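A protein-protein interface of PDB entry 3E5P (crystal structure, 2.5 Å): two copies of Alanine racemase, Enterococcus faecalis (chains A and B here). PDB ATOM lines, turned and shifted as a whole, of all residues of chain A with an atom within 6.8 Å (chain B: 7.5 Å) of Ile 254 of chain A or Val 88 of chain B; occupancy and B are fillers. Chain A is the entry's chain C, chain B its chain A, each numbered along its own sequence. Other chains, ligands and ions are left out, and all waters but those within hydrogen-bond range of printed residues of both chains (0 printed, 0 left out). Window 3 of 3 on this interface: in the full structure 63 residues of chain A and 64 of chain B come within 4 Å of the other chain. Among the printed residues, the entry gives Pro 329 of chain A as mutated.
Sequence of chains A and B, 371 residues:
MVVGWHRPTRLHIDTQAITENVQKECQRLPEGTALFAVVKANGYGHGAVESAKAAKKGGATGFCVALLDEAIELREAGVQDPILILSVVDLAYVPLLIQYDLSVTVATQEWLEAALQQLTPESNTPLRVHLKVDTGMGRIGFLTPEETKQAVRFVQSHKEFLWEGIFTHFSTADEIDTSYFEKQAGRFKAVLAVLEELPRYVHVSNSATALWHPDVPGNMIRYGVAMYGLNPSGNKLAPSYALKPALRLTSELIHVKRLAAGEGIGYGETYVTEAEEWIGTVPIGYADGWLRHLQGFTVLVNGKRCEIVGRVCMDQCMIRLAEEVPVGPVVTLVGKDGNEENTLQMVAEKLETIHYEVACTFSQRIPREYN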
ATOM      1  N   ARG A   7      12.151  12.526  -6.583  1.00  0.00           N
ATOM      2  CA  ARG A   7      11.925  12.892  -7.969  1.00  0.00           C
ATOM      3  C   ARG A   7      11.894  14.422  -8.057  1.00  0.00           C
ATOM      4  O   ARG A   7      11.295  15.088  -7.215  1.00  0.00           O
ATOM      5  CB  ARG A   7      10.609  12.296  -8.444  1.00  0.00           C
ATOM      6  CG  ARG A   7      10.406  12.417  -9.928  1.00  0.00           C
ATOM      7  CD  ARG A   7       9.020  11.981 -10.304  1.00  0.00           C
ATOM      8  NE  ARG A   7       8.016  12.783  -9.623  1.00  0.00           N
ATOM      9  CZ  ARG A   7       6.712  12.607  -9.778  1.00  0.00           C
ATOM     10  NH1 ARG A   7       6.287  11.655 -10.594  1.00  0.00           N
ATOM     11  NH2 ARG A   7       5.841  13.374  -9.123  1.00  0.00           N
ATOM     12  N   PRO A   8      12.536  14.998  -9.086  1.00  0.00           N
ATOM     13  CA  PRO A   8      12.592  16.455  -9.272  1.00  0.00           C
ATOM     14  C   PRO A   8      11.277  17.241  -9.383  1.00  0.00           C
ATOM     15  O   PRO A   8      11.270  18.461  -9.209  1.00  0.00           O
ATOM     16  CB  PRO A   8      13.473  16.605 -10.509  1.00  0.00           C
ATOM     17  CG  PRO A   8      13.174  15.364 -11.285  1.00  0.00           C
ATOM     18  CD  PRO A   8      13.183  14.305 -10.213  1.00  0.00           C
ATOM     19  N   SER A 251       9.527  21.157 -12.268  1.00  0.00           N
ATOM     20  CA  SER A 251      10.092  19.847 -12.593  1.00  0.00           C
ATOM     21  C   SER A 251      11.454  20.066 -13.235  1.00  0.00           C
ATOM     22  O   SER A 251      12.020  21.152 -13.112  1.00  0.00           O
ATOM     23  CB  SER A 251       9.190  19.054 -13.539  1.00  0.00           C
ATOM     24  OG  SER A 251       9.577  17.688 -13.560  1.00  0.00           O
ATOM     25  N   GLU A 252      11.982  19.060 -13.921  1.00  0.00           N
ATOM     26  CA  GLU A 252      13.290  19.206 -14.530  1.00  0.00           C
ATOM     27  C   GLU A 252      13.551  18.200 -15.643  1.00  0.00           C
ATOM     28  O   GLU A 252      13.049  17.081 -15.605  1.00  0.00           O
ATOM     29  CB  GLU A 252      14.372  19.091 -13.443  1.00  0.00           C
ATOM     30  CG  GLU A 252      15.443  18.025 -13.688  1.00  0.00           C
ATOM     31  CD  GLU A 252      16.555  18.020 -12.626  1.00  0.00           C
ATOM     32  OE1 GLU A 252      17.530  17.250 -12.795  1.00  0.00           O
ATOM     33  OE2 GLU A 252      16.456  18.776 -11.624  1.00  0.00           O
ATOM     34  N   LEU A 253      14.330  18.612 -16.640  1.00  0.00           N
ATOM     35  CA  LEU A 253      14.675  17.729 -17.749  1.00  0.00           C
ATOM     36  C   LEU A 253      15.546  16.630 -17.164  1.00  0.00           C
ATOM     37  O   LEU A 253      16.500  16.917 -16.446  1.00  0.00           O
ATOM     38  CB  LEU A 253      15.474  18.481 -18.821  1.00  0.00           C
ATOM     39  CG  LEU A 253      14.821  19.648 -19.576  1.00  0.00           C
ATOM     40  CD1 LEU A 253      15.819  20.223 -20.575  1.00  0.00           C
ATOM     41  CD2 LEU A 253      13.550  19.180 -20.298  1.00  0.00           C
ATOM     42  N   ILE A 254      15.224  15.375 -17.441  1.00  0.00           N
ATOM     43  CA  ILE A 254      16.040  14.295 -16.913  1.00  0.00           C
ATOM     44  C   ILE A 254      16.633  13.485 -18.048  1.00  0.00           C
ATOM     45  O   ILE A 254      17.211  12.424 -17.834  1.00  0.00           O
ATOM     46  CB  ILE A 254      15.231  13.361 -16.010  1.00  0.00           C
ATOM     47  CG1 ILE A 254      14.035  12.802 -16.782  1.00  0.00           C
ATOM     48  CG2 ILE A 254      14.798  14.103 -14.759  1.00  0.00           C
ATOM     49  CD1 ILE A 254      13.339  11.676 -16.062  1.00  0.00           C
ATOM     50  N   HIS A 255      16.487  14.000 -19.258  1.00  0.00           N
ATOM     51  CA  HIS A 255      17.007  13.335 -20.434  1.00  0.00           C
ATOM     52  C   HIS A 255      16.800  14.262 -21.613  1.00  0.00           C
ATOM     53  O   HIS A 255      15.718  14.810 -21.792  1.00  0.00           O
ATOM     54  CB  HIS A 255      16.279  12.006 -20.660  1.00  0.00           C
ATOM     55  CG  HIS A 255      16.867  11.169 -21.755  1.00  0.00           C
ATOM     56  ND1 HIS A 255      16.243  10.984 -22.971  1.00  0.00           N
ATOM     57  CD2 HIS A 255      18.021  10.462 -21.816  1.00  0.00           C
ATOM     58  CE1 HIS A 255      16.986  10.200 -23.734  1.00  0.00           C
ATOM     59  NE2 HIS A 255      18.069   9.869 -23.056  1.00  0.00           N
ATOM     60  N   VAL A 256      17.855  14.452 -22.396  1.00  0.00           N
ATOM     61  CA  VAL A 256      17.800  15.306 -23.572  1.00  0.00           C
ATOM     62  C   VAL A 256      18.469  14.566 -24.704  1.00  0.00           C
ATOM     63  O   VAL A 256      19.578  14.060 -24.548  1.00  0.00           O
ATOM     64  CB  VAL A 256      18.547  16.630 -23.358  1.00  0.00           C
ATOM     65  CG1 VAL A 256      18.359  17.529 -24.562  1.00  0.00           C
ATOM     66  CG2 VAL A 256      18.040  17.318 -22.105  1.00  0.00           C
ATOM     67  N   GLY A 280      13.405  16.770 -24.909  1.00  0.00           N
ATOM     68  CA  GLY A 280      13.699  16.604 -23.496  1.00  0.00           C
ATOM     69  C   GLY A 280      12.604  15.858 -22.758  1.00  0.00           C
ATOM     70  O   GLY A 280      11.420  16.053 -23.030  1.00  0.00           O
ATOM     71  N   THR A 281      12.994  15.003 -21.819  1.00  0.00           N
ATOM     72  CA  THR A 281      12.037  14.216 -21.047  1.00  0.00           C
ATOM     73  C   THR A 281      11.782  14.827 -19.676  1.00  0.00           C
ATOM     74  O   THR A 281      12.710  15.088 -18.912  1.00  0.00           O
ATOM     75  CB  THR A 281      12.531  12.780 -20.860  1.00  0.00           C
ATOM     76  OG1 THR A 281      12.541  12.122 -22.131  1.00  0.00           O
ATOM     77  CG2 THR A 281      11.626  12.017 -19.903  1.00  0.00           C
ATOM     78  N   VAL A 282      10.510  15.039 -19.366  1.00  0.00           N
ATOM     79  CA  VAL A 282      10.119  15.629 -18.102  1.00  0.00           C
ATOM     80  C   VAL A 282       9.404  14.586 -17.259  1.00  0.00           C
ATOM     81  O   VAL A 282       8.474  13.941 -17.735  1.00  0.00           O
ATOM     82  CB  VAL A 282       9.190  16.800 -18.346  1.00  0.00           C
ATOM     83  CG1 VAL A 282       8.897  17.505 -17.031  1.00  0.00           C
ATOM     84  CG2 VAL A 282       9.818  17.743 -19.362  1.00  0.00           C
ATOM     85  N   PRO A 283       9.822  14.420 -15.987  1.00  0.00           N
ATOM     86  CA  PRO A 283       9.245  13.449 -15.046  1.00  0.00           C
ATOM     87  C   PRO A 283       7.916  13.813 -14.354  1.00  0.00           C
ATOM     88  O   PRO A 283       7.842  13.875 -13.125  1.00  0.00           O
ATOM     89  CB  PRO A 283      10.379  13.237 -14.046  1.00  0.00           C
ATOM     90  CG  PRO A 283      10.952  14.628 -13.937  1.00  0.00           C
ATOM     91  CD  PRO A 283      10.962  15.132 -15.374  1.00  0.00           C
ATOM     92  N   GLN A 316       5.409  10.788 -17.333  1.00  0.00           N
ATOM     93  CA  GLN A 316       6.284  11.749 -18.000  1.00  0.00           C
ATOM     94  C   GLN A 316       5.785  12.197 -19.369  1.00  0.00           C
ATOM     95  O   GLN A 316       4.900  11.573 -19.949  1.00  0.00           O
ATOM     96  CB  GLN A 316       7.686  11.159 -18.139  1.00  0.00           C
ATOM     97  CG  GLN A 316       7.718   9.843 -18.855  1.00  0.00           C
ATOM     98  CD  GLN A 316       8.717   8.878 -18.252  1.00  0.00           C
ATOM     99  OE1 GLN A 316       8.857   7.745 -18.719  1.00  0.00           O
ATOM    100  NE2 GLN A 316       9.417   9.315 -17.207  1.00  0.00           N
ATOM    101  N   VAL A 327      20.777  18.113 -19.361  1.00  0.00           N
ATOM    102  CA  VAL A 327      19.658  17.698 -18.530  1.00  0.00           C
ATOM    103  C   VAL A 327      19.917  18.433 -17.232  1.00  0.00           C
ATOM    104  O   VAL A 327      21.063  18.759 -16.939  1.00  0.00           O
ATOM    105  CB  VAL A 327      19.669  16.179 -18.258  1.00  0.00           C
ATOM    106  CG1 VAL A 327      19.599  15.418 -19.560  1.00  0.00           C
ATOM    107  CG2 VAL A 327      20.921  15.794 -17.488  1.00  0.00           C
ATOM    108  N   GLY A 328      18.870  18.725 -16.470  1.00  0.00           N
ATOM    109  CA  GLY A 328      19.073  19.408 -15.203  1.00  0.00           C
ATOM    110  C   GLY A 328      18.408  20.763 -15.079  1.00  0.00           C
ATOM    111  O   GLY A 328      17.972  21.136 -13.985  1.00  0.00           O
ATOM    112  N   PRO A 329      18.344  21.545 -16.166  1.00  0.00           N
ATOM    113  CA  PRO A 329      17.692  22.844 -16.017  1.00  0.00           C
ATOM    114  C   PRO A 329      16.238  22.656 -15.582  1.00  0.00           C
ATOM    115  O   PRO A 329      15.549  21.745 -16.051  1.00  0.00           O
ATOM    116  CB  PRO A 329      17.845  23.470 -17.408  1.00  0.00           C
ATOM    117  CG  PRO A 329      18.015  22.299 -18.318  1.00  0.00           C
ATOM    118  CD  PRO A 329      18.895  21.381 -17.521  1.00  0.00           C
ATOM    119  N   VAL A 331      12.295  22.955 -15.168  1.00  0.00           N
ATOM    120  CA  VAL A 331      11.177  23.130 -16.077  1.00  0.00           C
ATOM    121  C   VAL A 331       9.995  23.698 -15.308  1.00  0.00           C
ATOM    122  O   VAL A 331       9.493  23.061 -14.384  1.00  0.00           O
ATOM    123  CB  VAL A 331      10.756  21.787 -16.706  1.00  0.00           C
ATOM    124  CG1 VAL A 331       9.706  22.027 -17.784  1.00  0.00           C
ATOM    125  CG2 VAL A 331      11.985  21.067 -17.282  1.00  0.00           C
ATOM    126  N   ALA B  66       7.635   3.009 -11.371  1.00  0.00           N
ATOM    127  CA  ALA B  66       8.118   4.154 -12.140  1.00  0.00           C
ATOM    128  C   ALA B  66       9.049   5.033 -11.307  1.00  0.00           C
ATOM    129  O   ALA B  66       9.990   5.637 -11.833  1.00  0.00           O
ATOM    130  CB  ALA B  66       6.947   4.976 -12.646  1.00  0.00           C
ATOM    131  N   LEU B  67       8.783   5.099 -10.006  1.00  0.00           N
ATOM    132  CA  LEU B  67       9.587   5.920  -9.117  1.00  0.00           C
ATOM    133  C   LEU B  67      10.376   5.156  -8.051  1.00  0.00           C
ATOM    134  O   LEU B  67       9.913   4.142  -7.517  1.00  0.00           O
ATOM    135  CB  LEU B  67       8.697   6.943  -8.406  1.00  0.00           C
ATOM    136  CG  LEU B  67       7.928   7.932  -9.278  1.00  0.00           C
ATOM    137  CD1 LEU B  67       7.309   9.000  -8.388  1.00  0.00           C
ATOM    138  CD2 LEU B  67       8.869   8.561 -10.295  1.00  0.00           C
ATOM    139  N   LEU B  68      11.567   5.666  -7.747  1.00  0.00           N
ATOM    140  CA  LEU B  68      12.399   5.094  -6.711  1.00  0.00           C
ATOM    141  C   LEU B  68      11.557   5.011  -5.432  1.00  0.00           C
ATOM    142  O   LEU B  68      11.567   4.004  -4.735  1.00  0.00           O
ATOM    143  CB  LEU B  68      13.611   5.992  -6.474  1.00  0.00           C
ATOM    144  CG  LEU B  68      14.388   5.725  -5.185  1.00  0.00           C
ATOM    145  CD1 LEU B  68      14.831   4.269  -5.164  1.00  0.00           C
ATOM    146  CD2 LEU B  68      15.576   6.677  -5.079  1.00  0.00           C
ATOM    147  N   ILE B  85      12.857  -0.273 -11.635  1.00  0.00           N
ATOM    148  CA  ILE B  85      12.453   1.121 -11.755  1.00  0.00           C
ATOM    149  C   ILE B  85      12.563   1.397 -13.254  1.00  0.00           C
ATOM    150  O   ILE B  85      13.646   1.321 -13.839  1.00  0.00           O
ATOM    151  CB  ILE B  85      13.390   2.037 -10.950  1.00  0.00           C
ATOM    152  CG1 ILE B  85      13.316   1.652  -9.470  1.00  0.00           C
ATOM    153  CG2 ILE B  85      12.991   3.491 -11.138  1.00  0.00           C
ATOM    154  CD1 ILE B  85      14.469   2.144  -8.630  1.00  0.00           C
ATOM    155  N   LEU B  86      11.427   1.684 -13.877  1.00  0.00           N
ATOM    156  CA  LEU B  86      11.375   1.920 -15.315  1.00  0.00           C
ATOM    157  C   LEU B  86      11.915   3.255 -15.806  1.00  0.00           C
ATOM    158  O   LEU B  86      12.133   3.428 -16.995  1.00  0.00           O
ATOM    159  CB  LEU B  86       9.940   1.726 -15.819  1.00  0.00           C
ATOM    160  CG  LEU B  86       9.413   0.304 -15.612  1.00  0.00           C
ATOM    161  CD1 LEU B  86       7.945   0.218 -16.023  1.00  0.00           C
ATOM    162  CD2 LEU B  86      10.271  -0.680 -16.414  1.00  0.00           C
ATOM    163  N   SER B  87      12.143   4.194 -14.904  1.00  0.00           N
ATOM    164  CA  SER B  87      12.660   5.498 -15.309  1.00  0.00           C
ATOM    165  C   SER B  87      14.140   5.608 -14.939  1.00  0.00           C
ATOM    166  O   SER B  87      14.703   4.683 -14.358  1.00  0.00           O
ATOM    167  CB  SER B  87      11.878   6.610 -14.601  1.00  0.00           C
ATOM    168  OG  SER B  87      10.476   6.418 -14.734  1.00  0.00           O
ATOM    169  N   VAL B  88      14.774   6.728 -15.279  1.00  0.00           N
ATOM    170  CA  VAL B  88      16.173   6.915 -14.908  1.00  0.00           C
ATOM    171  C   VAL B  88      16.174   7.477 -13.482  1.00  0.00           C
ATOM    172  O   VAL B  88      15.371   8.351 -13.144  1.00  0.00           O
ATOM    173  CB  VAL B  88      16.922   7.903 -15.862  1.00  0.00           C
ATOM    174  CG1 VAL B  88      16.896   7.378 -17.278  1.00  0.00           C
ATOM    175  CG2 VAL B  88      16.297   9.283 -15.804  1.00  0.00           C
ATOM    176  N   VAL B  89      17.059   6.952 -12.643  1.00  0.00           N
ATOM    177  CA  VAL B  89      17.157   7.397 -11.261  1.00  0.00           C
ATOM    178  C   VAL B  89      18.357   8.321 -11.086  1.00  0.00           C
ATOM    179  O   VAL B  89      19.478   7.962 -11.425  1.00  0.00           O
ATOM    180  CB  VAL B  89      17.293   6.192 -10.323  1.00  0.00           C
ATOM    181  CG1 VAL B  89      17.553   6.658  -8.899  1.00  0.00           C
ATOM    182  CG2 VAL B  89      16.029   5.356 -10.386  1.00  0.00           C
ATOM    183  N   ASP B  90      18.117   9.511 -10.551  1.00  0.00           N
ATOM    184  CA  ASP B  90      19.184  10.482 -10.353  1.00  0.00           C
ATOM    185  C   ASP B  90      20.368   9.817  -9.673  1.00  0.00           C
ATOM    186  O   ASP B  90      20.203   9.100  -8.684  1.00  0.00           O
ATOM    187  CB  ASP B  90      18.694  11.650  -9.499  1.00  0.00           C
ATOM    188  CG  ASP B  90      19.595  12.871  -9.601  1.00  0.00           C
ATOM    189  OD1 ASP B  90      20.825  12.732  -9.407  1.00  0.00           O
ATOM    190  OD2 ASP B  90      19.067  13.974  -9.870  1.00  0.00           O
ATOM    191  N   LEU B  91      21.558  10.064 -10.209  1.00  0.00           N
ATOM    192  CA  LEU B  91      22.790   9.494  -9.683  1.00  0.00           C
ATOM    193  C   LEU B  91      22.930   9.525  -8.161  1.00  0.00           C
ATOM    194  O   LEU B  91      23.324   8.531  -7.547  1.00  0.00           O
ATOM    195  CB  LEU B  91      23.982  10.192 -10.333  1.00  0.00           C
ATOM    196  CG  LEU B  91      24.200   9.794 -11.797  1.00  0.00           C
ATOM    197  CD1 LEU B  91      25.120  10.782 -12.495  1.00  0.00           C
ATOM    198  CD2 LEU B  91      24.782   8.383 -11.845  1.00  0.00           C
ATOM    199  N   VAL B 104      17.662  -1.011 -11.882  1.00  0.00           N
ATOM    200  CA  VAL B 104      17.489   0.309 -12.452  1.00  0.00           C
ATOM    201  C   VAL B 104      17.651   0.346 -13.947  1.00  0.00           C
ATOM    202  O   VAL B 104      18.432  -0.400 -14.524  1.00  0.00           O
ATOM    203  CB  VAL B 104      18.498   1.298 -11.874  1.00  0.00           C
ATOM    204  CG1 VAL B 104      18.301   2.665 -12.497  1.00  0.00           C
ATOM    205  CG2 VAL B 104      18.335   1.375 -10.380  1.00  0.00           C
ATOM    206  N   THR B 105      16.900   1.246 -14.563  1.00  0.00           N
ATOM    207  CA  THR B 105      16.950   1.446 -15.995  1.00  0.00           C
ATOM    208  C   THR B 105      18.121   2.372 -16.225  1.00  0.00           C
ATOM    209  O   THR B 105      18.382   3.235 -15.400  1.00  0.00           O
ATOM    210  CB  THR B 105      15.673   2.155 -16.490  1.00  0.00           C
ATOM    211  OG1 THR B 105      14.529   1.338 -16.205  1.00  0.00           O
ATOM    212  CG2 THR B 105      15.756   2.432 -17.979  1.00  0.00           C
ATOM    213  N   VAL B 106      18.824   2.181 -17.334  1.00  0.00           N
ATOM    214  CA  VAL B 106      19.951   3.035 -17.711  1.00  0.00           C
ATOM    215  C   VAL B 106      19.763   3.370 -19.190  1.00  0.00           C
ATOM    216  O   VAL B 106      19.715   2.479 -20.027  1.00  0.00           O
ATOM    217  CB  VAL B 106      21.314   2.321 -17.496  1.00  0.00           C
ATOM    218  CG1 VAL B 106      21.315   0.993 -18.204  1.00  0.00           C
ATOM    219  CG2 VAL B 106      22.444   3.174 -18.033  1.00  0.00           C
ATOM    220  N   ALA B 107      19.646   4.652 -19.510  1.00  0.00           N
ATOM    221  CA  ALA B 107      19.425   5.063 -20.890  1.00  0.00           C
ATOM    222  C   ALA B 107      20.570   5.834 -21.536  1.00  0.00           C
ATOM    223  O   ALA B 107      20.457   6.250 -22.691  1.00  0.00           O
ATOM    224  CB  ALA B 107      18.146   5.891 -20.977  1.00  0.00           C
ATOM    225  N   THR B 108      21.664   6.034 -20.808  1.00  0.00           N
ATOM    226  CA  THR B 108      22.804   6.770 -21.351  1.00  0.00           C
ATOM    227  C   THR B 108      24.123   6.194 -20.867  1.00  0.00           C
ATOM    228  O   THR B 108      24.171   5.512 -19.844  1.00  0.00           O
ATOM    229  CB  THR B 108      22.748   8.255 -20.954  1.00  0.00           C
ATOM    230  OG1 THR B 108      22.636   8.369 -19.530  1.00  0.00           O
ATOM    231  CG2 THR B 108      21.555   8.935 -21.613  1.00  0.00           C
ATOM    232  N   TRP B 111      25.789   8.036 -17.472  1.00  0.00           N
ATOM    233  CA  TRP B 111      25.208   7.644 -16.200  1.00  0.00           C
ATOM    234  C   TRP B 111      25.991   6.464 -15.621  1.00  0.00           C
ATOM    235  O   TRP B 111      26.303   6.428 -14.433  1.00  0.00           O
ATOM    236  CB  TRP B 111      23.750   7.246 -16.394  1.00  0.00           C
ATOM    237  CG  TRP B 111      22.970   7.225 -15.128  1.00  0.00           C
ATOM    238  CD1 TRP B 111      22.210   8.237 -14.620  1.00  0.00           C
ATOM    239  CD2 TRP B 111      22.854   6.133 -14.206  1.00  0.00           C
ATOM    240  NE1 TRP B 111      21.623   7.845 -13.440  1.00  0.00           N
ATOM    241  CE2 TRP B 111      22.003   6.557 -13.163  1.00  0.00           C
ATOM    242  CE3 TRP B 111      23.384   4.840 -14.162  1.00  0.00           C
ATOM    243  CZ2 TRP B 111      21.668   5.728 -12.085  1.00  0.00           C
ATOM    244  CZ3 TRP B 111      23.051   4.016 -13.091  1.00  0.00           C
ATOM    245  CH2 TRP B 111      22.199   4.465 -12.068  1.00  0.00           C
ATOM    246  N   ILE B 140      13.192   7.738 -23.721  1.00  0.00           N
ATOM    247  CA  ILE B 140      14.551   7.525 -23.220  1.00  0.00           C
ATOM    248  C   ILE B 140      15.226   6.303 -23.854  1.00  0.00           C
ATOM    249  O   ILE B 140      14.576   5.517 -24.545  1.00  0.00           O
ATOM    250  CB  ILE B 140      14.531   7.294 -21.701  1.00  0.00           C
ATOM    251  CG1 ILE B 140      13.673   6.056 -21.392  1.00  0.00           C
ATOM    252  CG2 ILE B 140      13.983   8.520 -20.993  1.00  0.00           C
ATOM    253  CD1 ILE B 140      13.663   5.617 -19.935  1.00  0.00           C
ATOM    254  N   GLY B 141      16.531   6.159 -23.607  1.00  0.00           N
ATOM    255  CA  GLY B 141      17.281   5.015 -24.110  1.00  0.00           C
ATOM    256  C   GLY B 141      18.314   5.198 -25.210  1.00  0.00           C
ATOM    257  O   GLY B 141      18.346   6.219 -25.888  1.00  0.00           O
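Hydrophobic or aromatic side chains of chain B within 4 Å of the printed part of chain A: Leu 67, Val 88 and Ile 140. Printed residues of chain A that touch a printed residue of chain B: Arg 7, Ile 254, His 255 and Gln 316. Hydrophobic or aromatic side chains of chain A that line the printed part of chain B: Ile 254 and His 255. Among the printed residues, 5 pairs touch across the chains. Among the printed residues, no Asp or Glu carboxylate lies within 4 Å of a Lys or Arg side-chain nitrogen of the other chain.
The side-chain hydroxyl (OG) of Ser 87 of chain B is in hydrogen-bond range of the backbone carbonyl oxygen (O) of Ala 66 of chain B, at 3.0 Å. The backbone NH (N) of Ile 254 of chain A lies within hydrogen-bond range of the backbone carbonyl oxygen (O) of Thr 281 of chain A (2.9 Å). The backbone NH (N) of Thr 281 of chain A lies within hydrogen-bond range of the backbone carbonyl oxygen (O) of His 255 of chain A (2.7 Å).
No position is printed for both chains. Of the 5 pairs that touch across the chains among the printed residues, none has its exchanged pair printed and touching as well.
CD of Arg 7 of chain A touches CD2 of Leu 67 of chain B, 3.4 Å away. Ile 254 of chain A touches Val 88 of chain B. His 255 of chain A touches Thr 108 of chain B. CE1 of His 255 of chain A touches CA of Ile 140 of chain B (3.7 Å). Ser 87 of chain B touches Gln 316 of chain A.
Of the printed residues of chain B, Ile 254 of chain A touches Val 88 (3.8 Å). Of chain A, only Ile 254 (3.8 Å) comes within 4 Å of Val 88 of chain B. Printed residues of chain B within 4 Å of His 255 of chain A: Thr 108 (3.9 Å) and Ile 140 (3.7 Å). Of the printed residues of chain A, Thr 108 of chain B touches His 255 (3.9 Å).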
